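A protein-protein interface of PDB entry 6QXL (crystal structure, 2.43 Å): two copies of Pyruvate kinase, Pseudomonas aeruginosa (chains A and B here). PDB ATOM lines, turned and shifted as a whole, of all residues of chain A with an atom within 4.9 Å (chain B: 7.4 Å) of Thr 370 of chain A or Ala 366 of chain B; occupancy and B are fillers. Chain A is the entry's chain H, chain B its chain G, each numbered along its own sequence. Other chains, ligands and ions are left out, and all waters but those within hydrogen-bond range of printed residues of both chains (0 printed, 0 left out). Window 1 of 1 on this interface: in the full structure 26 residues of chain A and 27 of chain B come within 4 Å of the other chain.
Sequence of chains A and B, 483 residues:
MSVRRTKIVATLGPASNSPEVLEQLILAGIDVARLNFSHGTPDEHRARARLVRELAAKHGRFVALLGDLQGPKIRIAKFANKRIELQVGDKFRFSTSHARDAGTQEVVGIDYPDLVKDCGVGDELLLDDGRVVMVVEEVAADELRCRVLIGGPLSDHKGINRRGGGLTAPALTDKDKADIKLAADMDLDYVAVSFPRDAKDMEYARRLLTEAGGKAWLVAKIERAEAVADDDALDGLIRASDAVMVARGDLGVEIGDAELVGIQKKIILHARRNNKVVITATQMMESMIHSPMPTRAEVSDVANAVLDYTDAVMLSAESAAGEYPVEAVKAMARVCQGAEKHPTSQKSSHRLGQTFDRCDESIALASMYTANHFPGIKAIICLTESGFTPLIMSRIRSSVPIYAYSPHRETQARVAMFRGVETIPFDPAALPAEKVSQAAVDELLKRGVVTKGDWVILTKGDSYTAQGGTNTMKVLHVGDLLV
Of the 23 printed residues of chain B, 11 touch a printed residue of chain A. Hydrophobic or aromatic side chains of chain B within 4 Å of the printed part of chain A: His 350, Phe 356, Ile 363, Leu 365, Ala 366, Tyr 369 and Met 473. Along chain B the printed residues that touch a printed residue of chain A span positions 350 to 473. Hydrophobic or aromatic side chains of chain A that line the printed part of chain B: Ala 366, Tyr 369, His 373, Phe 374, Met 473 and Val 475. Among the printed residues, no Asp or Glu carboxylate lies within 4 Å of a Lys or Arg side-chain nitrogen of the other chain.
The backbone carbonyl oxygen (O) of His 350 of chain B sits at hydrogen-bond distance from the side-chain hydroxyl (OH) of Tyr 369 of chain A (2.7 Å). The backbone NH (N) of Phe 356 of chain B sits at hydrogen-bond distance from the backbone carbonyl oxygen (O) of His 373 of chain A (3.0 Å). SG of Cys 359 of chain B sits close to O of Val 475 of chain A (3.7 Å). O of Met 473 of chain B sits at hydrogen-bond distance from N of Met 473 of chain A (2.9 Å).
A ring nitrogen (NE2) of His 350 of chain B lies close to the side-chain amide nitrogen (ND2) of Asn 372 of chain B, at 3.3 Å. NE of Arg 358 of chain B is in salt-bridge range of OD1 of Asp 360 of chain B, at 3.3 Å. The side-chain hydroxyl (OG) of Ser 362 of chain B lies within hydrogen-bond range of the backbone carbonyl oxygen (O) of Arg 358 of chain B, at 3.1 Å. O of Ala 366 of chain B is in hydrogen-bond range of OG1 of Thr 370 of chain B (2.8 Å). OG of Ser 367 of chain A is in hydrogen-bond range of SD of Met 473 of chain A (3.6 Å). ND1 of His 373 of chain A lies within hydrogen-bond range of O of Tyr 369 of chain A (2.8 Å).
Among the printed residues, pairs that only touch across the chains: Ala 366 of chain A with Tyr 369 of chain B, Ala 366 of chain A with Thr 370 of chain B, Ala 366 of chain A with Met 473 of chain B, Tyr 369 of chain A with Phe 356 of chain B, Tyr 369 of chain A with Leu 365 of chain B, Tyr 369 of chain A with Ala 366 of chain B, Tyr 369 of chain A with Tyr 369 of chain B, Thr 370 of chain A with Ala 366 of chain B, Phe 374 of chain A with Phe 356 of chain B, Phe 374 of chain A with Arg 358 of chain B, Phe 374 of chain A with Ser 362 of chain B, Met 473 of chain A with Ile 363 of chain B, Met 473 of chain A with Ala 366 of chain B and Val 475 of chain A with Ile 363 of chain B.
Of the printed residues of chain B, Ala 366 of chain A touches Tyr 369 (3.9 Å), Thr 370 (3.2 Å) and Met 473 (3.8 Å). Of chain B, only Ala 366 (3.2 Å) comes within 4 Å of Thr 370 of chain A. Printed residues of chain A within 4 Å of His 350 of chain B: Tyr 369 (2.7 Å). Of the printed residues of chain A, Phe 356 of chain B touches Tyr 369, His 373 and Phe 374. Printed residues of chain A within 4 Å of Arg 358 of chain B: Phe 374 (3.9 Å). Asp 360 of chain B touches none of the printed residues of chain A. Of the printed residues of chain A, Ala 366 of chain B touches Tyr 369, Thr 370 and Met 473. Asn 372 of chain B touches none of the printed residues of chain A. The nearest residue of chain B that does not touch Thr 370 of chain A is Ser 362 of chain B (4.1 Å). The nearest printed residue of chain A that does not touch Ala 366 of chain B is Ala 366 of chain A (4.5 Å).
Ala 366 of chain A touches Thr 370 of chain B, and with the chains exchanged Thr 370 of chain A touches Ala 366 of chain B. Ala 366 of chain A touches Met 473 of chain B, and with the chains exchanged Met 473 of chain A touches Ala 366 of chain B. Tyr 369 of chain B touches its own counterpart, Tyr 369 of chain A. Met 473 of chain A touches its own counterpart, Met 473 of chain B. Positions printed for both chains: 366, 367, 368, 369, 370, 371, 372, 457 and 473. Of the 18 pairs that touch across the chains among the printed residues, 8 have their exchanged pair printed and touching as well.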
ATOM      1  N   ALA A 366      16.377  10.509  21.064  1.00  0.00           N
ATOM      2  CA  ALA A 366      17.708  10.320  21.597  1.00  0.00           C
ATOM      3  C   ALA A 366      18.026   8.852  21.827  1.00  0.00           C
ATOM      4  O   ALA A 366      19.179   8.423  21.674  1.00  0.00           O
ATOM      5  CB  ALA A 366      17.877  11.109  22.877  1.00  0.00           C
ATOM      6  N   SER A 367      17.003   8.077  22.186  1.00  0.00           N
ATOM      7  CA  SER A 367      17.182   6.647  22.414  1.00  0.00           C
ATOM      8  C   SER A 367      17.413   5.910  21.118  1.00  0.00           C
ATOM      9  O   SER A 367      18.280   5.019  21.060  1.00  0.00           O
ATOM     10  CB  SER A 367      15.971   6.053  23.128  1.00  0.00           C
ATOM     11  OG  SER A 367      15.687   6.748  24.323  1.00  0.00           O
ATOM     12  N   MET A 368      16.656   6.262  20.083  1.00  0.00           N
ATOM     13  CA  MET A 368      16.876   5.614  18.783  1.00  0.00           C
ATOM     14  C   MET A 368      18.254   5.931  18.239  1.00  0.00           C
ATOM     15  O   MET A 368      18.952   5.032  17.764  1.00  0.00           O
ATOM     16  CB  MET A 368      15.784   5.999  17.786  1.00  0.00           C
ATOM     17  CG  MET A 368      14.402   5.534  18.229  1.00  0.00           C
ATOM     18  SD  MET A 368      14.326   3.825  18.794  1.00  0.00           S
ATOM     19  CE  MET A 368      14.510   2.950  17.260  1.00  0.00           C
ATOM     20  N   TYR A 369      18.672   7.193  18.360  1.00  0.00           N
ATOM     21  CA  TYR A 369      20.048   7.565  18.024  1.00  0.00           C
ATOM     22  C   TYR A 369      21.056   6.720  18.793  1.00  0.00           C
ATOM     23  O   TYR A 369      21.966   6.144  18.209  1.00  0.00           O
ATOM     24  CB  TYR A 369      20.281   9.036  18.303  1.00  0.00           C
ATOM     25  CG  TYR A 369      21.712   9.486  18.188  1.00  0.00           C
ATOM     26  CD1 TYR A 369      22.280   9.787  16.953  1.00  0.00           C
ATOM     27  CD2 TYR A 369      22.493   9.645  19.329  1.00  0.00           C
ATOM     28  CE1 TYR A 369      23.583  10.233  16.862  1.00  0.00           C
ATOM     29  CE2 TYR A 369      23.803  10.110  19.236  1.00  0.00           C
ATOM     30  CZ  TYR A 369      24.335  10.401  18.007  1.00  0.00           C
ATOM     31  OH  TYR A 369      25.635  10.824  17.952  1.00  0.00           O
ATOM     32  N   THR A 370      20.885   6.632  20.099  1.00  0.00           N
ATOM     33  CA  THR A 370      21.842   5.897  20.902  1.00  0.00           C
ATOM     34  C   THR A 370      21.873   4.415  20.521  1.00  0.00           C
ATOM     35  O   THR A 370      22.952   3.839  20.334  1.00  0.00           O
ATOM     36  CB  THR A 370      21.530   6.055  22.392  1.00  0.00           C
ATOM     37  OG1 THR A 370      21.555   7.449  22.715  1.00  0.00           O
ATOM     38  CG2 THR A 370      22.549   5.318  23.236  1.00  0.00           C
ATOM     39  N   ALA A 371      20.697   3.813  20.386  1.00  0.00           N
ATOM     40  CA  ALA A 371      20.608   2.383  20.071  1.00  0.00           C
ATOM     41  C   ALA A 371      21.179   2.053  18.704  1.00  0.00           C
ATOM     42  O   ALA A 371      21.866   1.041  18.543  1.00  0.00           O
ATOM     43  CB  ALA A 371      19.160   1.890  20.161  1.00  0.00           C
ATOM     44  N   ASN A 372      20.923   2.913  17.728  1.00  0.00           N
ATOM     45  CA  ASN A 372      21.455   2.687  16.387  1.00  0.00           C
ATOM     46  C   ASN A 372      22.963   2.807  16.299  1.00  0.00           C
ATOM     47  O   ASN A 372      23.519   2.356  15.320  1.00  0.00           O
ATOM     48  CB  ASN A 372      20.801   3.617  15.353  1.00  0.00           C
ATOM     49  CG  ASN A 372      19.494   3.074  14.816  1.00  0.00           C
ATOM     50  OD1 ASN A 372      18.990   2.043  15.271  1.00  0.00           O
ATOM     51  ND2 ASN A 372      18.930   3.770  13.846  1.00  0.00           N
ATOM     52  N   HIS A 373      23.629   3.420  17.283  1.00  0.00           N
ATOM     53  CA  HIS A 373      25.080   3.586  17.221  1.00  0.00           C
ATOM     54  C   HIS A 373      25.885   2.789  18.234  1.00  0.00           C
ATOM     55  O   HIS A 373      27.053   2.553  17.982  1.00  0.00           O
ATOM     56  CB  HIS A 373      25.429   5.049  17.288  1.00  0.00           C
ATOM     57  CG  HIS A 373      24.942   5.827  16.107  1.00  0.00           C
ATOM     58  ND1 HIS A 373      23.685   6.398  16.058  1.00  0.00           N
ATOM     59  CD2 HIS A 373      25.528   6.112  14.915  1.00  0.00           C
ATOM     60  CE1 HIS A 373      23.524   7.009  14.898  1.00  0.00           C
ATOM     61  NE2 HIS A 373      24.628   6.857  14.191  1.00  0.00           N
ATOM     62  N   PHE A 374      25.296   2.399  19.363  1.00  0.00           N
ATOM     63  CA  PHE A 374      25.982   1.564  20.341  1.00  0.00           C
ATOM     64  C   PHE A 374      25.431   0.140  20.169  1.00  0.00           C
ATOM     65  O   PHE A 374      24.406  -0.195  20.736  1.00  0.00           O
ATOM     66  CB  PHE A 374      25.792   2.149  21.762  1.00  0.00           C
ATOM     67  CG  PHE A 374      26.549   1.411  22.896  1.00  0.00           C
ATOM     68  CD1 PHE A 374      27.803   0.818  22.709  1.00  0.00           C
ATOM     69  CD2 PHE A 374      26.010   1.390  24.187  1.00  0.00           C
ATOM     70  CE1 PHE A 374      28.452   0.169  23.768  1.00  0.00           C
ATOM     71  CE2 PHE A 374      26.670   0.767  25.245  1.00  0.00           C
ATOM     72  CZ  PHE A 374      27.893   0.177  25.042  1.00  0.00           C
ATOM     73  N   ILE A 377      23.765  -2.390  22.701  1.00  0.00           N
ATOM     74  CA  ILE A 377      22.373  -2.271  23.098  1.00  0.00           C
ATOM     75  C   ILE A 377      21.528  -3.269  22.317  1.00  0.00           C
ATOM     76  O   ILE A 377      21.513  -3.246  21.099  1.00  0.00           O
ATOM     77  CB  ILE A 377      21.850  -0.846  22.886  1.00  0.00           C
ATOM     78  CG1 ILE A 377      22.497   0.054  23.935  1.00  0.00           C
ATOM     79  CG2 ILE A 377      20.331  -0.776  22.958  1.00  0.00           C
ATOM     80  CD1 ILE A 377      22.445   1.529  23.576  1.00  0.00           C
ATOM     81  N   ILE A 457      18.598   0.066  26.979  1.00  0.00           N
ATOM     82  CA  ILE A 457      18.167   1.421  27.261  1.00  0.00           C
ATOM     83  C   ILE A 457      16.857   1.367  28.015  1.00  0.00           C
ATOM     84  O   ILE A 457      15.961   0.627  27.646  1.00  0.00           O
ATOM     85  CB  ILE A 457      17.984   2.232  25.969  1.00  0.00           C
ATOM     86  CG1 ILE A 457      19.358   2.547  25.369  1.00  0.00           C
ATOM     87  CG2 ILE A 457      17.233   3.543  26.232  1.00  0.00           C
ATOM     88  CD1 ILE A 457      19.228   3.238  24.003  1.00  0.00           C
ATOM     89  N   MET A 473      16.632   8.919  30.132  1.00  0.00           N
ATOM     90  CA  MET A 473      17.157   7.812  29.352  1.00  0.00           C
ATOM     91  C   MET A 473      18.321   7.260  30.116  1.00  0.00           C
ATOM     92  O   MET A 473      19.212   8.005  30.465  1.00  0.00           O
ATOM     93  CB  MET A 473      17.630   8.323  27.973  1.00  0.00           C
ATOM     94  CG  MET A 473      18.149   7.235  27.045  1.00  0.00           C
ATOM     95  SD  MET A 473      18.914   7.814  25.524  1.00  0.00           S
ATOM     96  CE  MET A 473      20.619   7.801  26.065  1.00  0.00           C
ATOM     97  N   VAL A 475      21.249   3.965  30.323  1.00  0.00           N
ATOM     98  CA  VAL A 475      21.891   2.870  29.621  1.00  0.00           C
ATOM     99  C   VAL A 475      22.447   1.925  30.675  1.00  0.00           C
ATOM    100  O   VAL A 475      23.328   2.303  31.453  1.00  0.00           O
ATOM    101  CB  VAL A 475      23.002   3.413  28.685  1.00  0.00           C
ATOM    102  CG1 VAL A 475      23.782   2.281  28.012  1.00  0.00           C
ATOM    103  CG2 VAL A 475      22.386   4.326  27.628  1.00  0.00           C
ATOM    104  N   HIS B 350      27.097  14.422  13.968  1.00  0.00           N
ATOM    105  CA  HIS B 350      26.851  13.558  15.126  1.00  0.00           C
ATOM    106  C   HIS B 350      27.387  12.148  15.013  1.00  0.00           C
ATOM    107  O   HIS B 350      26.815  11.211  15.583  1.00  0.00           O
ATOM    108  CB  HIS B 350      25.383  13.591  15.585  1.00  0.00           C
ATOM    109  CG  HIS B 350      24.932  14.932  16.051  1.00  0.00           C
ATOM    110  ND1 HIS B 350      25.130  15.432  17.326  1.00  0.00           N
ATOM    111  CD2 HIS B 350      24.326  15.913  15.353  1.00  0.00           C
ATOM    112  CE1 HIS B 350      24.665  16.657  17.379  1.00  0.00           C
ATOM    113  NE2 HIS B 350      24.148  16.989  16.216  1.00  0.00           N
ATOM    114  N   PHE B 356      29.983   3.134  18.515  1.00  0.00           N
ATOM    115  CA  PHE B 356      30.447   3.588  19.830  1.00  0.00           C
ATOM    116  C   PHE B 356      31.008   2.408  20.615  1.00  0.00           C
ATOM    117  O   PHE B 356      30.615   1.255  20.410  1.00  0.00           O
ATOM    118  CB  PHE B 356      29.328   4.290  20.620  1.00  0.00           C
ATOM    119  CG  PHE B 356      28.679   5.437  19.889  1.00  0.00           C
ATOM    120  CD1 PHE B 356      29.256   5.985  18.697  1.00  0.00           C
ATOM    121  CD2 PHE B 356      27.493   5.999  20.383  1.00  0.00           C
ATOM    122  CE1 PHE B 356      28.645   7.052  18.031  1.00  0.00           C
ATOM    123  CE2 PHE B 356      26.891   7.069  19.711  1.00  0.00           C
ATOM    124  CZ  PHE B 356      27.472   7.596  18.541  1.00  0.00           C
ATOM    125  N   ARG B 358      31.754   2.707  24.354  1.00  0.00           N
ATOM    126  CA  ARG B 358      31.469   2.718  25.790  1.00  0.00           C
ATOM    127  C   ARG B 358      30.093   3.281  26.042  1.00  0.00           C
ATOM    128  O   ARG B 358      29.507   3.916  25.193  1.00  0.00           O
ATOM    129  CB  ARG B 358      32.472   3.574  26.539  1.00  0.00           C
ATOM    130  CG  ARG B 358      33.841   2.935  26.838  1.00  0.00           C
ATOM    131  CD  ARG B 358      34.797   4.008  27.286  1.00  0.00           C
ATOM    132  NE  ARG B 358      34.816   4.127  28.754  1.00  0.00           N
ATOM    133  CZ  ARG B 358      35.715   4.824  29.454  1.00  0.00           C
ATOM    134  NH1 ARG B 358      35.747   4.760  30.783  1.00  0.00           N
ATOM    135  NH2 ARG B 358      36.641   5.612  28.885  1.00  0.00           N
ATOM    136  N   CYS B 359      29.622   3.050  27.249  1.00  0.00           N
ATOM    137  CA  CYS B 359      28.336   3.529  27.681  1.00  0.00           C
ATOM    138  C   CYS B 359      28.365   5.025  28.016  1.00  0.00           C
ATOM    139  O   CYS B 359      27.426   5.758  27.670  1.00  0.00           O
ATOM    140  CB  CYS B 359      27.863   2.723  28.901  1.00  0.00           C
ATOM    141  SG  CYS B 359      26.474   3.431  29.856  1.00  0.00           S
ATOM    142  N   ASP B 360      29.409   5.475  28.709  1.00  0.00           N
ATOM    143  CA  ASP B 360      29.471   6.899  29.084  1.00  0.00           C
ATOM    144  C   ASP B 360      29.701   7.767  27.856  1.00  0.00           C
ATOM    145  O   ASP B 360      29.103   8.853  27.750  1.00  0.00           O
ATOM    146  CB  ASP B 360      30.511   7.179  30.193  1.00  0.00           C
ATOM    147  CG  ASP B 360      31.871   6.538  29.942  1.00  0.00           C
ATOM    148  OD1 ASP B 360      32.066   5.873  28.891  1.00  0.00           O
ATOM    149  OD2 ASP B 360      32.709   6.740  30.850  1.00  0.00           O
ATOM    150  N   GLU B 361      30.521   7.254  26.915  1.00  0.00           N
ATOM    151  CA  GLU B 361      30.631   7.862  25.588  1.00  0.00           C
ATOM    152  C   GLU B 361      29.241   8.052  24.978  1.00  0.00           C
ATOM    153  O   GLU B 361      28.922   9.124  24.485  1.00  0.00           O
ATOM    154  CB  GLU B 361      31.522   7.006  24.690  1.00  0.00           C
ATOM    155  CG  GLU B 361      32.123   7.660  23.454  1.00  0.00           C
ATOM    156  CD  GLU B 361      33.216   6.741  22.850  1.00  0.00           C
ATOM    157  OE1 GLU B 361      33.109   6.294  21.664  1.00  0.00           O
ATOM    158  OE2 GLU B 361      34.166   6.412  23.614  1.00  0.00           O
ATOM    159  N   SER B 362      28.407   7.023  25.054  1.00  0.00           N
ATOM    160  CA  SER B 362      27.066   7.067  24.458  1.00  0.00           C
ATOM    161  C   SER B 362      26.157   8.129  25.037  1.00  0.00           C
ATOM    162  O   SER B 362      25.427   8.782  24.294  1.00  0.00           O
ATOM    163  CB  SER B 362      26.379   5.706  24.541  1.00  0.00           C
ATOM    164  OG  SER B 362      26.994   4.834  23.579  1.00  0.00           O
ATOM    165  N   ILE B 363      26.208   8.317  26.344  1.00  0.00           N
ATOM    166  CA  ILE B 363      25.383   9.337  26.979  1.00  0.00           C
ATOM    167  C   ILE B 363      25.864  10.721  26.590  1.00  0.00           C
ATOM    168  O   ILE B 363      25.055  11.631  26.379  1.00  0.00           O
ATOM    169  CB  ILE B 363      25.389   9.206  28.528  1.00  0.00           C
ATOM    170  CG1 ILE B 363      24.805   7.859  28.965  1.00  0.00           C
ATOM    171  CG2 ILE B 363      24.611  10.346  29.177  1.00  0.00           C
ATOM    172  CD1 ILE B 363      23.297   7.789  28.839  1.00  0.00           C
ATOM    173  N   ALA B 364      27.179  10.897  26.506  1.00  0.00           N
ATOM    174  CA  ALA B 364      27.715  12.184  26.063  1.00  0.00           C
ATOM    175  C   ALA B 364      27.231  12.506  24.656  1.00  0.00           C
ATOM    176  O   ALA B 364      26.644  13.575  24.414  1.00  0.00           O
ATOM    177  CB  ALA B 364      29.223  12.184  26.115  1.00  0.00           C
ATOM    178  N   LEU B 365      27.411  11.552  23.741  1.00  0.00           N
ATOM    179  CA  LEU B 365      26.998  11.770  22.355  1.00  0.00           C
ATOM    180  C   LEU B 365      25.500  11.995  22.259  1.00  0.00           C
ATOM    181  O   LEU B 365      25.053  12.879  21.525  1.00  0.00           O
ATOM    182  CB  LEU B 365      27.440  10.627  21.470  1.00  0.00           C
ATOM    183  CG  LEU B 365      28.981  10.564  21.412  1.00  0.00           C
ATOM    184  CD1 LEU B 365      29.501   9.392  20.622  1.00  0.00           C
ATOM    185  CD2 LEU B 365      29.604  11.828  20.868  1.00  0.00           C
ATOM    186  N   ALA B 366      24.730  11.233  23.032  1.00  0.00           N
ATOM    187  CA  ALA B 366      23.286  11.357  23.001  1.00  0.00           C
ATOM    188  C   ALA B 366      22.824  12.713  23.480  1.00  0.00           C
ATOM    189  O   ALA B 366      21.813  13.239  22.997  1.00  0.00           O
ATOM    190  CB  ALA B 366      22.648  10.251  23.817  1.00  0.00           C
ATOM    191  N   SER B 367      23.557  13.297  24.425  1.00  0.00           N
ATOM    192  CA  SER B 367      23.215  14.617  24.947  1.00  0.00           C
ATOM    193  C   SER B 367      23.493  15.696  23.923  1.00  0.00           C
ATOM    194  O   SER B 367      22.687  16.618  23.758  1.00  0.00           O
ATOM    195  CB  SER B 367      23.996  14.914  26.227  1.00  0.00           C
ATOM    196  OG  SER B 367      23.808  13.907  27.195  1.00  0.00           O
ATOM    197  N   MET B 368      24.626  15.598  23.239  1.00  0.00           N
ATOM    198  CA  MET B 368      24.929  16.591  22.193  1.00  0.00           C
ATOM    199  C   MET B 368      23.918  16.510  21.058  1.00  0.00           C
ATOM    200  O   MET B 368      23.428  17.549  20.603  1.00  0.00           O
ATOM    201  CB  MET B 368      26.345  16.432  21.680  1.00  0.00           C
ATOM    202  CG  MET B 368      27.385  16.666  22.751  1.00  0.00           C
ATOM    203  SD  MET B 368      27.126  18.153  23.749  1.00  0.00           S
ATOM    204  CE  MET B 368      27.554  19.426  22.573  1.00  0.00           C
ATOM    205  N   TYR B 369      23.559  15.294  20.653  1.00  0.00           N
ATOM    206  CA  TYR B 369      22.464  15.109  19.698  1.00  0.00           C
ATOM    207  C   TYR B 369      21.191  15.770  20.185  1.00  0.00           C
ATOM    208  O   TYR B 369      20.569  16.540  19.454  1.00  0.00           O
ATOM    209  CB  TYR B 369      22.221  13.630  19.440  1.00  0.00           C
ATOM    210  CG  TYR B 369      20.987  13.315  18.644  1.00  0.00           C
ATOM    211  CD1 TYR B 369      20.984  13.390  17.257  1.00  0.00           C
ATOM    212  CD2 TYR B 369      19.812  12.907  19.289  1.00  0.00           C
ATOM    213  CE1 TYR B 369      19.841  13.078  16.533  1.00  0.00           C
ATOM    214  CE2 TYR B 369      18.670  12.609  18.562  1.00  0.00           C
ATOM    215  CZ  TYR B 369      18.693  12.695  17.191  1.00  0.00           C
ATOM    216  OH  TYR B 369      17.558  12.393  16.491  1.00  0.00           O
ATOM    217  N   THR B 370      20.804  15.492  21.417  1.00  0.00           N
ATOM    218  CA  THR B 370      19.559  16.041  21.928  1.00  0.00           C
ATOM    219  C   THR B 370      19.601  17.565  21.975  1.00  0.00           C
ATOM    220  O   THR B 370      18.669  18.233  21.527  1.00  0.00           O
ATOM    221  CB  THR B 370      19.248  15.469  23.313  1.00  0.00           C
ATOM    222  OG1 THR B 370      19.181  14.051  23.228  1.00  0.00           O
ATOM    223  CG2 THR B 370      17.940  16.001  23.829  1.00  0.00           C
ATOM    224  N   ALA B 371      20.693  18.110  22.509  1.00  0.00           N
ATOM    225  CA  ALA B 371      20.818  19.563  22.655  1.00  0.00           C
ATOM    226  C   ALA B 371      20.840  20.287  21.317  1.00  0.00           C
ATOM    227  O   ALA B 371      20.234  21.341  21.169  1.00  0.00           O
ATOM    228  CB  ALA B 371      22.050  19.909  23.464  1.00  0.00           C
ATOM    229  N   ASN B 372      21.524  19.711  20.343  1.00  0.00           N
ATOM    230  CA  ASN B 372      21.574  20.328  19.015  1.00  0.00           C
ATOM    231  C   ASN B 372      20.248  20.324  18.285  1.00  0.00           C
ATOM    232  O   ASN B 372      20.118  21.051  17.330  1.00  0.00           O
ATOM    233  CB  ASN B 372      22.659  19.668  18.127  1.00  0.00           C
ATOM    234  CG  ASN B 372      24.030  20.282  18.355  1.00  0.00           C
ATOM    235  OD1 ASN B 372      24.243  21.103  19.251  1.00  0.00           O
ATOM    236  ND2 ASN B 372      24.961  19.877  17.551  1.00  0.00           N
ATOM    237  N   ILE B 380      23.908  22.238  29.426  1.00  0.00           N
ATOM    238  CA  ILE B 380      24.124  20.851  29.786  1.00  0.00           C
ATOM    239  C   ILE B 380      24.832  20.824  31.140  1.00  0.00           C
ATOM    240  O   ILE B 380      25.934  21.347  31.272  1.00  0.00           O
ATOM    241  CB  ILE B 380      24.978  20.138  28.762  1.00  0.00           C
ATOM    242  CG1 ILE B 380      24.246  20.145  27.401  1.00  0.00           C
ATOM    243  CG2 ILE B 380      25.321  18.722  29.277  1.00  0.00           C
ATOM    244  CD1 ILE B 380      24.814  19.200  26.362  1.00  0.00           C
ATOM    245  N   MET B 393      31.577  15.134  25.297  1.00  0.00           N
ATOM    246  CA  MET B 393      30.555  16.066  24.824  1.00  0.00           C
ATOM    247  C   MET B 393      31.173  17.137  23.923  1.00  0.00           C
ATOM    248  O   MET B 393      30.625  17.456  22.868  1.00  0.00           O
ATOM    249  CB  MET B 393      29.827  16.726  25.980  1.00  0.00           C
ATOM    250  CG  MET B 393      29.012  15.796  26.852  1.00  0.00           C
ATOM    251  SD  MET B 393      28.167  16.729  28.133  1.00  0.00           S
ATOM    252  CE  MET B 393      27.195  15.423  28.881  1.00  0.00           C
ATOM    253  N   ILE B 396      31.964  17.260  19.967  1.00  0.00           N
ATOM    254  CA  ILE B 396      30.890  17.390  19.001  1.00  0.00           C
ATOM    255  C   ILE B 396      30.598  18.852  18.763  1.00  0.00           C
ATOM    256  O   ILE B 396      30.453  19.615  19.707  1.00  0.00           O
ATOM    257  CB  ILE B 396      29.614  16.684  19.525  1.00  0.00           C
ATOM    258  CG1 ILE B 396      29.879  15.219  19.800  1.00  0.00           C
ATOM    259  CG2 ILE B 396      28.470  16.815  18.540  1.00  0.00           C
ATOM    260  CD1 ILE B 396      30.413  14.468  18.598  1.00  0.00           C
ATOM    261  N   ILE B 457      19.746  19.806  30.183  1.00  0.00           N
ATOM    262  CA  ILE B 457      20.090  18.391  30.205  1.00  0.00           C
ATOM    263  C   ILE B 457      20.971  18.141  31.420  1.00  0.00           C
ATOM    264  O   ILE B 457      21.906  18.899  31.667  1.00  0.00           O
ATOM    265  CB  ILE B 457      20.846  17.959  28.940  1.00  0.00           C
ATOM    266  CG1 ILE B 457      19.884  17.965  27.749  1.00  0.00           C
ATOM    267  CG2 ILE B 457      21.470  16.572  29.114  1.00  0.00           C
ATOM    268  CD1 ILE B 457      20.530  17.580  26.432  1.00  0.00           C
ATOM    269  N   THR B 459      23.320  15.044  33.142  1.00  0.00           N
ATOM    270  CA  THR B 459      23.884  13.710  33.012  1.00  0.00           C
ATOM    271  C   THR B 459      24.591  13.318  34.288  1.00  0.00           C
ATOM    272  O   THR B 459      25.182  14.162  34.954  1.00  0.00           O
ATOM    273  CB  THR B 459      24.900  13.599  31.834  1.00  0.00           C
ATOM    274  OG1 THR B 459      26.070  14.377  32.101  1.00  0.00           O
ATOM    275  CG2 THR B 459      24.263  14.055  30.518  1.00  0.00           C
ATOM    276  N   MET B 473      20.718  10.310  31.309  1.00  0.00           N
ATOM    277  CA  MET B 473      20.501  11.612  30.699  1.00  0.00           C
ATOM    278  C   MET B 473      19.092  11.996  31.045  1.00  0.00           C
ATOM    279  O   MET B 473      18.179  11.234  30.780  1.00  0.00           O
ATOM    280  CB  MET B 473      20.655  11.535  29.174  1.00  0.00           C
ATOM    281  CG  MET B 473      20.498  12.859  28.452  1.00  0.00           C
ATOM    282  SD  MET B 473      20.466  12.694  26.628  1.00  0.00           S
ATOM    283  CE  MET B 473      18.696  12.550  26.349  1.00  0.00           C
